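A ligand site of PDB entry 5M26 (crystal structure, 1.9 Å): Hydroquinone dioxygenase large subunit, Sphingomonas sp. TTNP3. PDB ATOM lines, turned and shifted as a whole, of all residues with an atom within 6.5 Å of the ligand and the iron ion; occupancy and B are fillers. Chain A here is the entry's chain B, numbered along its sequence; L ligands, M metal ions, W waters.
The side-chain carboxylate (OE2) of Glu 250 lies within hydrogen-bond range of an oxygen (O1) of the ligand (2.6 Å).
The iron ion is bound by OE2 of Glu 264, O2 of the ligand, NE2 of His 305, ND1 of His 258 and water W1. The iron ion has five donor atoms within binding distance.
Water W1 bridges OE1 of Glu 264 and OE1 of Glu 319.
The side-chain carboxylate of Glu 264 lies within hydrogen-bond range of the side-chain amide nitrogen of Asn 260, 2.5 Å away. The backbone NH of Met 299 is in hydrogen-bond range of the backbone carbonyl oxygen of Glu 264 (2.8 Å). A ring nitrogen (ND1) of His 305 sits close to the side-chain sulfur of Met 299 (3.8 Å). The side-chain carboxylate (OE1) of Glu 250 sits at hydrogen-bond distance from the backbone NH (N) of Trp 232 (2.9 Å). The side-chain hydroxyl (OG1) of Thr 248 sits at hydrogen-bond distance from the side-chain carboxylate (OE1) of Glu 250 (3.0 Å). The backbone carbonyl oxygen (O) of Ser 249 sits at hydrogen-bond distance from the backbone NH (N) of Trp 232, at 3.2 Å. N of Asn 233 lies within hydrogen-bond range of OG1 of Thr 248. The backbone NH (N) of Thr 248 is in hydrogen-bond range of the backbone carbonyl oxygen (O) of Leu 315, 2.9 Å away.
Merely in contact with the ligand: Phe 78 (2.9 Å), Trp 232 (3.1 Å), Trp 75 (3.2 Å), Pro 234 (3.4 Å), Asn 233 (3.5 Å), Leu 254 (3.5 Å), Thr 248 (3.6 Å), Phe 266 (3.7 Å), Val 317 (3.7 Å), Trp 275 (3.7 Å) and Leu 315 (3.9 Å). Hydrophobic or aromatic side chains that line the ligand: Trp 75, Phe 78, Trp 232, Pro 234, Leu 254, His 258, Phe 266, Trp 275, His 305, Leu 315 and Val 317. Within 4 Å of the ligand: Trp 75, Phe 78, Trp 232, Asn 233, Pro 234, Thr 248, Glu 250, Leu 254, His 258, Glu 264, Phe 266, Trp 275, His 305, Leu 315 and Val 317. The nearest printed residue that does not touch the ligand is Val 256 (4.7 Å).
The nearest printed residue that does not touch the iron ion is Phe 266 (4.03 Å).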
ATOM      1  N   TRP A  75      -1.549  24.231  28.425  1.00  0.00           N
ATOM      2  CA  TRP A  75      -1.269  23.687  27.083  1.00  0.00           C
ATOM      3  C   TRP A  75      -2.110  22.479  26.723  1.00  0.00           C
ATOM      4  O   TRP A  75      -1.957  21.914  25.630  1.00  0.00           O
ATOM      5  CB  TRP A  75       0.210  23.296  26.980  1.00  0.00           C
ATOM      6  CG  TRP A  75       1.171  24.394  27.228  1.00  0.00           C
ATOM      7  CD1 TRP A  75       0.951  25.745  27.122  1.00  0.00           C
ATOM      8  CD2 TRP A  75       2.546  24.241  27.603  1.00  0.00           C
ATOM      9  NE1 TRP A  75       2.104  26.431  27.436  1.00  0.00           N
ATOM     10  CE2 TRP A  75       3.095  25.541  27.733  1.00  0.00           C
ATOM     11  CE3 TRP A  75       3.364  23.131  27.871  1.00  0.00           C
ATOM     12  CZ2 TRP A  75       4.428  25.767  28.099  1.00  0.00           C
ATOM     13  CZ3 TRP A  75       4.700  23.350  28.221  1.00  0.00           C
ATOM     14  CH2 TRP A  75       5.206  24.681  28.338  1.00  0.00           C
ATOM     15  N   PHE A  78       0.006  19.700  25.810  1.00  0.00           N
ATOM     16  CA  PHE A  78       0.985  20.120  24.785  1.00  0.00           C
ATOM     17  C   PHE A  78       1.223  19.030  23.731  1.00  0.00           C
ATOM     18  O   PHE A  78       0.311  18.292  23.401  1.00  0.00           O
ATOM     19  CB  PHE A  78       2.293  20.613  25.470  1.00  0.00           C
ATOM     20  CG  PHE A  78       3.073  21.613  24.643  1.00  0.00           C
ATOM     21  CD1 PHE A  78       2.423  22.468  23.755  1.00  0.00           C
ATOM     22  CD2 PHE A  78       4.465  21.718  24.777  1.00  0.00           C
ATOM     23  CE1 PHE A  78       3.135  23.379  22.979  1.00  0.00           C
ATOM     24  CE2 PHE A  78       5.172  22.656  24.022  1.00  0.00           C
ATOM     25  CZ  PHE A  78       4.513  23.484  23.112  1.00  0.00           C
ATOM     26  N   THR A 231       4.318  34.024  30.849  1.00  0.00           N
ATOM     27  CA  THR A 231       5.614  33.630  30.274  1.00  0.00           C
ATOM     28  C   THR A 231       5.588  32.190  29.765  1.00  0.00           C
ATOM     29  O   THR A 231       4.855  31.366  30.316  1.00  0.00           O
ATOM     30  CB  THR A 231       6.743  33.792  31.300  1.00  0.00           C
ATOM     31  OG1 THR A 231       6.434  33.026  32.476  1.00  0.00           O
ATOM     32  CG2 THR A 231       6.855  35.262  31.696  1.00  0.00           C
ATOM     33  N   TRP A 232       6.367  31.891  28.727  1.00  0.00           N
ATOM     34  CA  TRP A 232       6.512  30.505  28.260  1.00  0.00           C
ATOM     35  C   TRP A 232       5.135  29.897  27.942  1.00  0.00           C
ATOM     36  O   TRP A 232       4.693  28.949  28.591  1.00  0.00           O
ATOM     37  CB  TRP A 232       7.263  29.648  29.285  1.00  0.00           C
ATOM     38  CG  TRP A 232       8.626  30.189  29.719  1.00  0.00           C
ATOM     39  CD1 TRP A 232       8.935  30.747  30.937  1.00  0.00           C
ATOM     40  CD2 TRP A 232       9.875  30.189  28.963  1.00  0.00           C
ATOM     41  NE1 TRP A 232      10.275  31.085  30.971  1.00  0.00           N
ATOM     42  CE2 TRP A 232      10.867  30.754  29.791  1.00  0.00           C
ATOM     43  CE3 TRP A 232      10.243  29.741  27.684  1.00  0.00           C
ATOM     44  CZ2 TRP A 232      12.206  30.912  29.375  1.00  0.00           C
ATOM     45  CZ3 TRP A 232      11.583  29.889  27.266  1.00  0.00           C
ATOM     46  CH2 TRP A 232      12.535  30.468  28.114  1.00  0.00           C
ATOM     47  N   ASN A 233       4.465  30.493  26.964  1.00  0.00           N
ATOM     48  CA  ASN A 233       3.133  30.087  26.580  1.00  0.00           C
ATOM     49  C   ASN A 233       2.919  30.214  25.067  1.00  0.00           C
ATOM     50  O   ASN A 233       2.250  31.118  24.612  1.00  0.00           O
ATOM     51  CB  ASN A 233       2.068  30.876  27.346  1.00  0.00           C
ATOM     52  CG  ASN A 233       0.680  30.225  27.272  1.00  0.00           C
ATOM     53  OD1 ASN A 233       0.558  28.992  27.294  1.00  0.00           O
ATOM     54  ND2 ASN A 233      -0.359  31.047  27.129  1.00  0.00           N
ATOM     55  N   PRO A 234       3.485  29.293  24.285  1.00  0.00           N
ATOM     56  CA  PRO A 234       3.344  29.382  22.825  1.00  0.00           C
ATOM     57  C   PRO A 234       1.860  29.514  22.469  1.00  0.00           C
ATOM     58  O   PRO A 234       1.042  28.730  22.952  1.00  0.00           O
ATOM     59  CB  PRO A 234       3.873  28.032  22.359  1.00  0.00           C
ATOM     60  CG  PRO A 234       4.898  27.673  23.393  1.00  0.00           C
ATOM     61  CD  PRO A 234       4.218  28.068  24.678  1.00  0.00           C
ATOM     62  N   THR A 248       5.532  33.881  21.844  1.00  0.00           N
ATOM     63  CA  THR A 248       5.338  33.943  23.308  1.00  0.00           C
ATOM     64  C   THR A 248       6.390  34.898  23.910  1.00  0.00           C
ATOM     65  O   THR A 248       7.386  35.210  23.249  1.00  0.00           O
ATOM     66  CB  THR A 248       5.367  32.508  23.933  1.00  0.00           C
ATOM     67  OG1 THR A 248       5.383  32.578  25.375  1.00  0.00           O
ATOM     68  CG2 THR A 248       6.561  31.681  23.430  1.00  0.00           C
ATOM     69  N   SER A 249       6.166  35.391  25.123  1.00  0.00           N
ATOM     70  CA  SER A 249       7.186  36.175  25.799  1.00  0.00           C
ATOM     71  C   SER A 249       7.820  35.336  26.893  1.00  0.00           C
ATOM     72  O   SER A 249       7.104  34.785  27.705  1.00  0.00           O
ATOM     73  CB  SER A 249       6.562  37.406  26.409  1.00  0.00           C
ATOM     74  OG  SER A 249       5.473  37.010  27.243  1.00  0.00           O
ATOM     75  N   GLU A 250       9.154  35.263  26.929  1.00  0.00           N
ATOM     76  CA  GLU A 250       9.860  34.314  27.796  1.00  0.00           C
ATOM     77  C   GLU A 250      10.730  35.083  28.778  1.00  0.00           C
ATOM     78  O   GLU A 250      11.407  36.022  28.391  1.00  0.00           O
ATOM     79  CB  GLU A 250      10.794  33.426  26.975  1.00  0.00           C
ATOM     80  CG  GLU A 250      10.243  32.919  25.634  1.00  0.00           C
ATOM     81  CD  GLU A 250       9.041  32.007  25.782  1.00  0.00           C
ATOM     82  OE1 GLU A 250       8.104  32.373  26.508  1.00  0.00           O
ATOM     83  OE2 GLU A 250       9.004  30.919  25.161  1.00  0.00           O
ATOM     84  N   LEU A 254      12.143  28.080  31.275  1.00  0.00           N
ATOM     85  CA  LEU A 254      10.992  27.279  30.826  1.00  0.00           C
ATOM     86  C   LEU A 254      10.722  26.262  31.943  1.00  0.00           C
ATOM     87  O   LEU A 254      11.657  25.562  32.341  1.00  0.00           O
ATOM     88  CB  LEU A 254      11.322  26.555  29.531  1.00  0.00           C
ATOM     89  CG  LEU A 254      10.225  25.603  29.041  1.00  0.00           C
ATOM     90  CD1 LEU A 254       8.913  26.351  28.779  1.00  0.00           C
ATOM     91  CD2 LEU A 254      10.749  24.925  27.782  1.00  0.00           C
ATOM     92  N   VAL A 256       9.432  23.456  32.196  1.00  0.00           N
ATOM     93  CA  VAL A 256       9.543  22.035  31.877  1.00  0.00           C
ATOM     94  C   VAL A 256      10.742  21.742  30.947  1.00  0.00           C
ATOM     95  O   VAL A 256      11.312  22.675  30.362  1.00  0.00           O
ATOM     96  CB  VAL A 256       8.255  21.519  31.211  1.00  0.00           C
ATOM     97  CG1 VAL A 256       7.013  21.821  32.087  1.00  0.00           C
ATOM     98  CG2 VAL A 256       8.098  22.091  29.792  1.00  0.00           C
ATOM     99  N   HIS A 258      10.922  20.021  27.473  1.00  0.00           N
ATOM    100  CA  HIS A 258       9.984  19.545  26.489  1.00  0.00           C
ATOM    101  C   HIS A 258      10.615  18.536  25.565  1.00  0.00           C
ATOM    102  O   HIS A 258      11.572  18.861  24.873  1.00  0.00           O
ATOM    103  CB  HIS A 258       9.458  20.681  25.666  1.00  0.00           C
ATOM    104  CG  HIS A 258       8.465  20.248  24.656  1.00  0.00           C
ATOM    105  ND1 HIS A 258       8.370  20.829  23.407  1.00  0.00           N
ATOM    106  CD2 HIS A 258       7.492  19.310  24.711  1.00  0.00           C
ATOM    107  CE1 HIS A 258       7.384  20.260  22.740  1.00  0.00           C
ATOM    108  NE2 HIS A 258       6.832  19.331  23.504  1.00  0.00           N
ATOM    109  N   GLY A 259      10.077  17.325  25.544  1.00  0.00           N
ATOM    110  CA  GLY A 259      10.569  16.301  24.597  1.00  0.00           C
ATOM    111  C   GLY A 259       9.479  16.125  23.552  1.00  0.00           C
ATOM    112  O   GLY A 259       8.557  15.343  23.758  1.00  0.00           O
ATOM    113  N   ASN A 260       9.572  16.851  22.448  1.00  0.00           N
ATOM    114  CA  ASN A 260       8.496  16.826  21.467  1.00  0.00           C
ATOM    115  C   ASN A 260       8.453  15.492  20.746  1.00  0.00           C
ATOM    116  O   ASN A 260       9.465  14.781  20.698  1.00  0.00           O
ATOM    117  CB  ASN A 260       8.631  17.964  20.461  1.00  0.00           C
ATOM    118  CG  ASN A 260       7.304  18.432  19.923  1.00  0.00           C
ATOM    119  OD1 ASN A 260       6.280  17.760  20.061  1.00  0.00           O
ATOM    120  ND2 ASN A 260       7.310  19.608  19.318  1.00  0.00           N
ATOM    121  N   GLU A 264      10.456  20.629  15.937  1.00  0.00           N
ATOM    122  CA  GLU A 264       9.856  21.959  16.097  1.00  0.00           C
ATOM    123  C   GLU A 264      10.940  23.019  15.938  1.00  0.00           C
ATOM    124  O   GLU A 264      12.124  22.719  16.078  1.00  0.00           O
ATOM    125  CB  GLU A 264       9.073  22.051  17.424  1.00  0.00           C
ATOM    126  CG  GLU A 264       9.901  22.536  18.571  1.00  0.00           C
ATOM    127  CD  GLU A 264       9.246  22.343  19.931  1.00  0.00           C
ATOM    128  OE1 GLU A 264       8.088  21.870  20.052  1.00  0.00           O
ATOM    129  OE2 GLU A 264       9.904  22.680  20.905  1.00  0.00           O
ATOM    130  N   PHE A 266      12.499  27.135  16.584  1.00  0.00           N
ATOM    131  CA  PHE A 266      12.530  28.364  17.361  1.00  0.00           C
ATOM    132  C   PHE A 266      13.140  29.483  16.545  1.00  0.00           C
ATOM    133  O   PHE A 266      14.300  29.380  16.098  1.00  0.00           O
ATOM    134  CB  PHE A 266      13.438  28.173  18.578  1.00  0.00           C
ATOM    135  CG  PHE A 266      12.938  27.205  19.588  1.00  0.00           C
ATOM    136  CD1 PHE A 266      11.570  27.035  19.808  1.00  0.00           C
ATOM    137  CD2 PHE A 266      13.835  26.472  20.368  1.00  0.00           C
ATOM    138  CE1 PHE A 266      11.104  26.142  20.766  1.00  0.00           C
ATOM    139  CE2 PHE A 266      13.382  25.588  21.330  1.00  0.00           C
ATOM    140  CZ  PHE A 266      11.995  25.423  21.526  1.00  0.00           C
ATOM    141  N   TRP A 275      19.214  27.505  25.191  1.00  0.00           N
ATOM    142  CA  TRP A 275      18.465  26.252  25.301  1.00  0.00           C
ATOM    143  C   TRP A 275      19.423  25.167  25.784  1.00  0.00           C
ATOM    144  O   TRP A 275      20.489  24.917  25.182  1.00  0.00           O
ATOM    145  CB  TRP A 275      17.863  25.836  23.952  1.00  0.00           C
ATOM    146  CG  TRP A 275      16.876  26.844  23.440  1.00  0.00           C
ATOM    147  CD1 TRP A 275      17.103  27.834  22.531  1.00  0.00           C
ATOM    148  CD2 TRP A 275      15.495  26.964  23.833  1.00  0.00           C
ATOM    149  NE1 TRP A 275      15.954  28.569  22.332  1.00  0.00           N
ATOM    150  CE2 TRP A 275      14.954  28.054  23.128  1.00  0.00           C
ATOM    151  CE3 TRP A 275      14.665  26.254  24.733  1.00  0.00           C
ATOM    152  CZ2 TRP A 275      13.620  28.458  23.262  1.00  0.00           C
ATOM    153  CZ3 TRP A 275      13.309  26.666  24.872  1.00  0.00           C
ATOM    154  CH2 TRP A 275      12.814  27.753  24.144  1.00  0.00           C
ATOM    155  N   MET A 299      14.731  22.066  16.920  1.00  0.00           N
ATOM    156  CA  MET A 299      14.900  21.140  17.991  1.00  0.00           C
ATOM    157  C   MET A 299      14.549  19.760  17.387  1.00  0.00           C
ATOM    158  O   MET A 299      13.376  19.529  17.049  1.00  0.00           O
ATOM    159  CB  MET A 299      13.947  21.441  19.153  1.00  0.00           C
ATOM    160  CG  MET A 299      14.280  22.659  20.025  1.00  0.00           C
ATOM    161  SD  MET A 299      15.896  22.493  20.823  1.00  0.00           S
ATOM    162  CE  MET A 299      16.824  23.643  19.815  1.00  0.00           C
ATOM    163  N   HIS A 305      14.331  19.892  25.564  1.00  0.00           N
ATOM    164  CA  HIS A 305      14.963  21.205  25.657  1.00  0.00           C
ATOM    165  C   HIS A 305      14.343  22.023  26.759  1.00  0.00           C
ATOM    166  O   HIS A 305      13.148  21.868  27.063  1.00  0.00           O
ATOM    167  CB  HIS A 305      14.844  21.955  24.326  1.00  0.00           C
ATOM    168  CG  HIS A 305      13.497  21.820  23.679  1.00  0.00           C
ATOM    169  ND1 HIS A 305      13.189  20.793  22.831  1.00  0.00           N
ATOM    170  CD2 HIS A 305      12.376  22.574  23.780  1.00  0.00           C
ATOM    171  CE1 HIS A 305      11.941  20.909  22.429  1.00  0.00           C
ATOM    172  NE2 HIS A 305      11.415  21.971  22.999  1.00  0.00           N
ATOM    173  N   LEU A 315       9.877  35.222  21.441  1.00  0.00           N
ATOM    174  CA  LEU A 315      10.283  33.982  20.756  1.00  0.00           C
ATOM    175  C   LEU A 315       9.129  33.530  19.881  1.00  0.00           C
ATOM    176  O   LEU A 315       7.981  33.576  20.309  1.00  0.00           O
ATOM    177  CB  LEU A 315      10.584  32.899  21.788  1.00  0.00           C
ATOM    178  CG  LEU A 315      10.768  31.477  21.260  1.00  0.00           C
ATOM    179  CD1 LEU A 315      12.101  31.329  20.504  1.00  0.00           C
ATOM    180  CD2 LEU A 315      10.677  30.537  22.454  1.00  0.00           C
ATOM    181  N   VAL A 317       7.686  30.204  18.404  1.00  0.00           N
ATOM    182  CA  VAL A 317       7.766  28.763  18.362  1.00  0.00           C
ATOM    183  C   VAL A 317       6.931  28.345  17.142  1.00  0.00           C
ATOM    184  O   VAL A 317       5.757  28.736  17.008  1.00  0.00           O
ATOM    185  CB  VAL A 317       7.229  28.110  19.657  1.00  0.00           C
ATOM    186  CG1 VAL A 317       7.173  26.583  19.541  1.00  0.00           C
ATOM    187  CG2 VAL A 317       8.114  28.500  20.833  1.00  0.00           C
ATOM    188  N   GLU A 319       5.304  25.267  15.031  1.00  0.00           N
ATOM    189  CA  GLU A 319       4.894  23.869  15.109  1.00  0.00           C
ATOM    190  C   GLU A 319       4.221  23.395  13.818  1.00  0.00           C
ATOM    191  O   GLU A 319       3.569  24.167  13.123  1.00  0.00           O
ATOM    192  CB  GLU A 319       3.880  23.619  16.241  1.00  0.00           C
ATOM    193  CG  GLU A 319       4.321  23.985  17.631  1.00  0.00           C
ATOM    194  CD  GLU A 319       5.244  22.971  18.293  1.00  0.00           C
ATOM    195  OE1 GLU A 319       5.758  23.337  19.371  1.00  0.00           O
ATOM    196  OE2 GLU A 319       5.447  21.828  17.808  1.00  0.00           O
HETATM  197  O1  LIG L   1       7.386  28.995  25.736  1.00  0.00           O
HETATM  198  C1  LIG L   1       7.799  27.795  25.295  1.00  0.00           C
HETATM  199  C2  LIG L   1       8.854  27.761  24.404  1.00  0.00           C
HETATM  200  C3  LIG L   1       9.296  26.530  23.923  1.00  0.00           C
HETATM  201  C4  LIG L   1       7.175  26.627  25.718  1.00  0.00           C
HETATM  202  C5  LIG L   1       7.619  25.390  25.222  1.00  0.00           C
HETATM  203  C6  LIG L   1       8.690  25.327  24.326  1.00  0.00           C
HETATM  204  O2  LIG L   1       9.139  24.130  23.832  1.00  0.00           O
HETATM  205  C7  LIG L   1       6.965  24.131  25.678  1.00  0.00           C
HETATM  206 FE    FE M   1       9.423  22.562  22.729  1.00  0.00          FE
HETATM  207  O   HOH W   1       7.363  23.584  21.867  1.00  0.00           O
